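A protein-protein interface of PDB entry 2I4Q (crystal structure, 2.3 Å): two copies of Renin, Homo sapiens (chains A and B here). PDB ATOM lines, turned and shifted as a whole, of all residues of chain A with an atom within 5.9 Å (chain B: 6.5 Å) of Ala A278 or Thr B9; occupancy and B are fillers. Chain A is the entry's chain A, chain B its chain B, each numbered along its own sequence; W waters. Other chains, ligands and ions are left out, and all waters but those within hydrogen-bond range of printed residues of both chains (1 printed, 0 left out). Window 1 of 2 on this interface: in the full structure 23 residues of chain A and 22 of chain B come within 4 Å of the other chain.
Among the printed residues, pairs that only touch across the chains: Ala A278 with Thr B9 (3.5 Å), Val A281 with Gln B166 (3.7 Å) and Ser A277 with Lys B30 (3.9 Å).
No position is printed for both chains.
Water W1 bridges NZ of Lys B30 (2.5 Å) and N of Ser A277 (3.2 Å).
Ala A278 touches just one residue of chain B: Thr B9 (3.5 Å). Thr B9 touches just one residue of chain A: Ala A278. Printed residues of chain B within 4 Å of Ser A277: Lys B30 (3.9 Å). Printed residues of chain B within 4 Å of Val A281: Gln B166. Printed residues of chain A within 4 Å of Gln B166: Val A281. The nearest residue of chain B that does not touch Ala A278 is Gln B166 (5.6 Å).
OG1 of Thr A276 sits close to N of Ala A278, 3.5 Å away. The backbone NH of Thr B9 lies within hydrogen-bond range of the backbone carbonyl oxygen of Tyr B17, at 2.8 Å. The backbone carbonyl oxygen (O) of Gly A258 lies close to the side-chain hydroxyl (OG) of Ser A277, 3.3 Å away.
Hydrophobic or aromatic side chains of chain A within 4 Å of the printed part of chain B: Ala A278. Of the 14 printed residues of chain B, 3 touch a printed residue of chain A. Among the printed residues, no Asp or Glu carboxylate lies within 4 Å of a Lys or Arg side-chain nitrogen of the other chain.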
ATOM      1  N   GLY A 258      20.527  21.504 -16.223  1.00  0.00           N
ATOM      2  CA  GLY A 258      20.165  21.409 -14.817  1.00  0.00           C
ATOM      3  C   GLY A 258      21.295  21.480 -13.803  1.00  0.00           C
ATOM      4  O   GLY A 258      21.256  22.321 -12.912  1.00  0.00           O
ATOM      5  N   THR A 276      21.711  24.200  -3.864  1.00  0.00           N
ATOM      6  CA  THR A 276      22.355  24.012  -5.164  1.00  0.00           C
ATOM      7  C   THR A 276      21.300  23.576  -6.170  1.00  0.00           C
ATOM      8  O   THR A 276      20.126  23.447  -5.832  1.00  0.00           O
ATOM      9  CB  THR A 276      23.464  22.945  -5.090  1.00  0.00           C
ATOM     10  OG1 THR A 276      22.906  21.690  -4.682  1.00  0.00           O
ATOM     11  CG2 THR A 276      24.501  23.287  -4.011  1.00  0.00           C
ATOM     12  N   SER A 277      21.722  23.340  -7.407  1.00  0.00           N
ATOM     13  CA  SER A 277      20.803  22.887  -8.442  1.00  0.00           C
ATOM     14  C   SER A 277      20.277  21.488  -8.122  1.00  0.00           C
ATOM     15  O   SER A 277      19.133  21.175  -8.421  1.00  0.00           O
ATOM     16  CB  SER A 277      21.467  22.926  -9.818  1.00  0.00           C
ATOM     17  OG  SER A 277      22.567  22.042  -9.892  1.00  0.00           O
ATOM     18  N   ALA A 278      21.101  20.668  -7.474  1.00  0.00           N
ATOM     19  CA  ALA A 278      20.685  19.335  -7.038  1.00  0.00           C
ATOM     20  C   ALA A 278      19.467  19.371  -6.110  1.00  0.00           C
ATOM     21  O   ALA A 278      18.698  18.418  -6.059  1.00  0.00           O
ATOM     22  CB  ALA A 278      21.848  18.618  -6.356  1.00  0.00           C
ATOM     23  N   ASP A 279      19.304  20.475  -5.381  1.00  0.00           N
ATOM     24  CA  ASP A 279      18.197  20.654  -4.440  1.00  0.00           C
ATOM     25  C   ASP A 279      16.892  21.164  -5.061  1.00  0.00           C
ATOM     26  O   ASP A 279      15.824  20.962  -4.481  1.00  0.00           O
ATOM     27  CB  ASP A 279      18.599  21.636  -3.333  1.00  0.00           C
ATOM     28  CG  ASP A 279      19.782  21.160  -2.525  1.00  0.00           C
ATOM     29  OD1 ASP A 279      19.751  20.016  -2.021  1.00  0.00           O
ATOM     30  OD2 ASP A 279      20.787  21.871  -2.339  1.00  0.00           O
ATOM     31  N   TYR A 280      16.957  21.850  -6.201  1.00  0.00           N
ATOM     32  CA  TYR A 280      15.741  22.448  -6.762  1.00  0.00           C
ATOM     33  C   TYR A 280      15.375  22.075  -8.195  1.00  0.00           C
ATOM     34  O   TYR A 280      14.375  22.559  -8.698  1.00  0.00           O
ATOM     35  CB  TYR A 280      15.750  23.975  -6.588  1.00  0.00           C
ATOM     36  CG  TYR A 280      16.725  24.742  -7.453  1.00  0.00           C
ATOM     37  CD1 TYR A 280      16.431  25.040  -8.782  1.00  0.00           C
ATOM     38  CD2 TYR A 280      17.925  25.212  -6.929  1.00  0.00           C
ATOM     39  CE1 TYR A 280      17.313  25.763  -9.567  1.00  0.00           C
ATOM     40  CE2 TYR A 280      18.813  25.935  -7.705  1.00  0.00           C
ATOM     41  CZ  TYR A 280      18.500  26.212  -9.020  1.00  0.00           C
ATOM     42  OH  TYR A 280      19.373  26.926  -9.789  1.00  0.00           O
ATOM     43  N   VAL A 281      16.153  21.229  -8.857  1.00  0.00           N
ATOM     44  CA  VAL A 281      15.713  20.690 -10.145  1.00  0.00           C
ATOM     45  C   VAL A 281      15.444  19.201  -9.986  1.00  0.00           C
ATOM     46  O   VAL A 281      16.182  18.492  -9.308  1.00  0.00           O
ATOM     47  CB  VAL A 281      16.678  21.000 -11.363  1.00  0.00           C
ATOM     48  CG1 VAL A 281      17.734  22.033 -11.021  1.00  0.00           C
ATOM     49  CG2 VAL A 281      17.319  19.743 -11.933  1.00  0.00           C
ATOM     50  N   ARG A 317      13.529  19.963   2.862  1.00  0.00           N
ATOM     51  CA  ARG A 317      14.355  18.798   2.525  1.00  0.00           C
ATOM     52  C   ARG A 317      15.821  19.038   2.853  1.00  0.00           C
ATOM     53  O   ARG A 317      16.497  18.149   3.358  1.00  0.00           O
ATOM     54  CB  ARG A 317      14.247  18.449   1.035  1.00  0.00           C
ATOM     55  CG  ARG A 317      13.297  17.321   0.724  1.00  0.00           C
ATOM     56  CD  ARG A 317      13.304  16.896  -0.731  1.00  0.00           C
ATOM     57  NE  ARG A 317      12.353  17.685  -1.522  1.00  0.00           N
ATOM     58  CZ  ARG A 317      12.652  18.343  -2.638  1.00  0.00           C
ATOM     59  NH1 ARG A 317      11.707  19.026  -3.271  1.00  0.00           N
ATOM     60  NH2 ARG A 317      13.886  18.327  -3.134  1.00  0.00           N
ATOM     61  N   ILE B   7      25.701  14.955   2.133  1.00  0.00           N
ATOM     62  CA  ILE B   7      24.996  14.342   1.013  1.00  0.00           C
ATOM     63  C   ILE B   7      25.719  14.692  -0.284  1.00  0.00           C
ATOM     64  O   ILE B   7      26.142  15.828  -0.487  1.00  0.00           O
ATOM     65  CB  ILE B   7      23.517  14.814   0.969  1.00  0.00           C
ATOM     66  CG1 ILE B   7      22.755  14.258   2.171  1.00  0.00           C
ATOM     67  CG2 ILE B   7      22.837  14.388  -0.339  1.00  0.00           C
ATOM     68  CD1 ILE B   7      21.513  15.048   2.522  1.00  0.00           C
ATOM     69  N   LEU B   8      25.848  13.700  -1.156  1.00  0.00           N
ATOM     70  CA  LEU B   8      26.589  13.837  -2.396  1.00  0.00           C
ATOM     71  C   LEU B   8      25.646  13.745  -3.585  1.00  0.00           C
ATOM     72  O   LEU B   8      24.602  13.096  -3.531  1.00  0.00           O
ATOM     73  CB  LEU B   8      27.663  12.746  -2.506  1.00  0.00           C
ATOM     74  CG  LEU B   8      28.634  12.608  -1.330  1.00  0.00           C
ATOM     75  CD1 LEU B   8      29.610  11.455  -1.580  1.00  0.00           C
ATOM     76  CD2 LEU B   8      29.391  13.915  -1.066  1.00  0.00           C
ATOM     77  N   THR B   9      26.044  14.400  -4.661  1.00  0.00           N
ATOM     78  CA  THR B   9      25.327  14.363  -5.920  1.00  0.00           C
ATOM     79  C   THR B   9      26.035  13.397  -6.854  1.00  0.00           C
ATOM     80  O   THR B   9      27.252  13.460  -6.993  1.00  0.00           O
ATOM     81  CB  THR B   9      25.330  15.766  -6.522  1.00  0.00           C
ATOM     82  OG1 THR B   9      24.611  16.655  -5.652  1.00  0.00           O
ATOM     83  CG2 THR B   9      24.579  15.803  -7.857  1.00  0.00           C
ATOM     84  N   ASN B  10      25.273  12.503  -7.481  1.00  0.00           N
ATOM     85  CA  ASN B  10      25.805  11.609  -8.498  1.00  0.00           C
ATOM     86  C   ASN B  10      25.500  12.139  -9.892  1.00  0.00           C
ATOM     87  O   ASN B  10      24.357  12.123 -10.323  1.00  0.00           O
ATOM     88  CB  ASN B  10      25.216  10.205  -8.346  1.00  0.00           C
ATOM     89  CG  ASN B  10      25.645   9.262  -9.466  1.00  0.00           C
ATOM     90  OD1 ASN B  10      26.277   9.681 -10.432  1.00  0.00           O
ATOM     91  ND2 ASN B  10      25.308   7.982  -9.333  1.00  0.00           N
ATOM     92  N   TYR B  11      26.534  12.584 -10.594  1.00  0.00           N
ATOM     93  CA  TYR B  11      26.428  12.946 -12.001  1.00  0.00           C
ATOM     94  C   TYR B  11      26.926  11.815 -12.905  1.00  0.00           C
ATOM     95  O   TYR B  11      28.123  11.565 -12.984  1.00  0.00           O
ATOM     96  CB  TYR B  11      27.244  14.213 -12.266  1.00  0.00           C
ATOM     97  CG  TYR B  11      27.240  14.654 -13.711  1.00  0.00           C
ATOM     98  CD1 TYR B  11      26.124  15.261 -14.264  1.00  0.00           C
ATOM     99  CD2 TYR B  11      28.352  14.465 -14.518  1.00  0.00           C
ATOM    100  CE1 TYR B  11      26.107  15.668 -15.595  1.00  0.00           C
ATOM    101  CE2 TYR B  11      28.353  14.872 -15.859  1.00  0.00           C
ATOM    102  CZ  TYR B  11      27.229  15.473 -16.384  1.00  0.00           C
ATOM    103  OH  TYR B  11      27.214  15.871 -17.692  1.00  0.00           O
ATOM    104  N   GLN B  15      31.073  11.232 -11.530  1.00  0.00           N
ATOM    105  CA  GLN B  15      31.445  12.327 -10.643  1.00  0.00           C
ATOM    106  C   GLN B  15      30.548  12.276  -9.421  1.00  0.00           C
ATOM    107  O   GLN B  15      29.343  12.082  -9.543  1.00  0.00           O
ATOM    108  CB  GLN B  15      31.293  13.687 -11.333  1.00  0.00           C
ATOM    109  CG  GLN B  15      31.914  13.786 -12.727  1.00  0.00           C
ATOM    110  CD  GLN B  15      31.941  15.219 -13.260  1.00  0.00           C
ATOM    111  OE1 GLN B  15      31.958  16.165 -12.484  1.00  0.00           O
ATOM    112  NE2 GLN B  15      31.942  15.373 -14.582  1.00  0.00           N
ATOM    113  N   TYR B  16      31.152  12.448  -8.253  1.00  0.00           N
ATOM    114  CA  TYR B  16      30.438  12.456  -6.989  1.00  0.00           C
ATOM    115  C   TYR B  16      30.991  13.599  -6.164  1.00  0.00           C
ATOM    116  O   TYR B  16      32.200  13.696  -5.955  1.00  0.00           O
ATOM    117  CB  TYR B  16      30.623  11.127  -6.240  1.00  0.00           C
ATOM    118  CG  TYR B  16      29.919   9.938  -6.867  1.00  0.00           C
ATOM    119  CD1 TYR B  16      30.529   9.193  -7.869  1.00  0.00           C
ATOM    120  CD2 TYR B  16      28.648   9.547  -6.442  1.00  0.00           C
ATOM    121  CE1 TYR B  16      29.904   8.098  -8.436  1.00  0.00           C
ATOM    122  CE2 TYR B  16      28.006   8.450  -7.009  1.00  0.00           C
ATOM    123  CZ  TYR B  16      28.643   7.727  -8.005  1.00  0.00           C
ATOM    124  OH  TYR B  16      28.027   6.635  -8.576  1.00  0.00           O
ATOM    125  N   TYR B  17      30.103  14.468  -5.700  1.00  0.00           N
ATOM    126  CA  TYR B  17      30.520  15.689  -5.022  1.00  0.00           C
ATOM    127  C   TYR B  17      29.446  16.215  -4.074  1.00  0.00           C
ATOM    128  O   TYR B  17      28.259  16.006  -4.292  1.00  0.00           O
ATOM    129  CB  TYR B  17      30.877  16.754  -6.059  1.00  0.00           C
ATOM    130  CG  TYR B  17      29.846  16.908  -7.149  1.00  0.00           C
ATOM    131  CD1 TYR B  17      29.917  16.152  -8.312  1.00  0.00           C
ATOM    132  CD2 TYR B  17      28.792  17.804  -7.014  1.00  0.00           C
ATOM    133  CE1 TYR B  17      28.968  16.282  -9.314  1.00  0.00           C
ATOM    134  CE2 TYR B  17      27.839  17.946  -8.019  1.00  0.00           C
ATOM    135  CZ  TYR B  17      27.936  17.183  -9.163  1.00  0.00           C
ATOM    136  OH  TYR B  17      26.997  17.312 -10.161  1.00  0.00           O
ATOM    137  N   GLY B  18      29.875  16.874  -3.005  1.00  0.00           N
ATOM    138  CA  GLY B  18      28.959  17.512  -2.073  1.00  0.00           C
ATOM    139  C   GLY B  18      29.412  18.920  -1.747  1.00  0.00           C
ATOM    140  O   GLY B  18      30.407  19.397  -2.282  1.00  0.00           O
ATOM    141  N   LYS B  30      30.982  22.958  -4.680  1.00  0.00           N
ATOM    142  CA  LYS B  30      30.789  21.533  -4.872  1.00  0.00           C
ATOM    143  C   LYS B  30      32.172  20.910  -4.955  1.00  0.00           C
ATOM    144  O   LYS B  30      32.975  21.319  -5.785  1.00  0.00           O
ATOM    145  CB  LYS B  30      30.022  21.278  -6.166  1.00  0.00           C
ATOM    146  CG  LYS B  30      28.618  21.867  -6.190  1.00  0.00           C
ATOM    147  CD  LYS B  30      28.125  22.060  -7.621  1.00  0.00           C
ATOM    148  CE  LYS B  30      26.599  22.099  -7.703  1.00  0.00           C
ATOM    149  NZ  LYS B  30      26.099  23.201  -8.588  1.00  0.00           N
ATOM    150  N   GLN B 166      14.793  11.357  -7.561  1.00  0.00           N
ATOM    151  CA  GLN B 166      15.646  12.433  -7.051  1.00  0.00           C
ATOM    152  C   GLN B 166      16.441  11.879  -5.876  1.00  0.00           C
ATOM    153  O   GLN B 166      16.519  12.479  -4.798  1.00  0.00           O
ATOM    154  CB  GLN B 166      14.800  13.640  -6.627  1.00  0.00           C
ATOM    155  CG  GLN B 166      13.848  14.139  -7.709  1.00  0.00           C
ATOM    156  CD  GLN B 166      14.500  14.176  -9.075  1.00  0.00           C
ATOM    157  OE1 GLN B 166      13.960  13.640 -10.050  1.00  0.00           O
ATOM    158  NE2 GLN B 166      15.675  14.792  -9.147  1.00  0.00           N
ATOM    159  N   LEU B 168      19.305   9.966  -3.368  1.00  0.00           N
ATOM    160  CA  LEU B 168      20.595  10.260  -2.785  1.00  0.00           C
ATOM    161  C   LEU B 168      21.670   9.836  -3.781  1.00  0.00           C
ATOM    162  O   LEU B 168      21.733   8.672  -4.183  1.00  0.00           O
ATOM    163  CB  LEU B 168      20.746   9.487  -1.472  1.00  0.00           C
ATOM    164  CG  LEU B 168      21.777  10.005  -0.475  1.00  0.00           C
ATOM    165  CD1 LEU B 168      21.308  11.311   0.135  1.00  0.00           C
ATOM    166  CD2 LEU B 168      22.023   8.965   0.609  1.00  0.00           C
ATOM    167  N   GLY B 169      22.490  10.789  -4.205  1.00  0.00           N
ATOM    168  CA  GLY B 169      23.630  10.484  -5.050  1.00  0.00           C
ATOM    169  C   GLY B 169      24.695   9.706  -4.294  1.00  0.00           C
ATOM    170  O   GLY B 169      25.450   8.943  -4.883  1.00  0.00           O
ATOM    171  N   GLY B 170      24.741   9.903  -2.980  1.00  0.00           N
ATOM    172  CA  GLY B 170      25.760   9.307  -2.139  1.00  0.00           C
ATOM    173  C   GLY B 170      25.919  10.051  -0.830  1.00  0.00           C
ATOM    174  O   GLY B 170      25.150  10.957  -0.524  1.00  0.00           O
HETATM  175  O   HOH W   1      24.292  24.971  -8.332  1.00  0.00           O
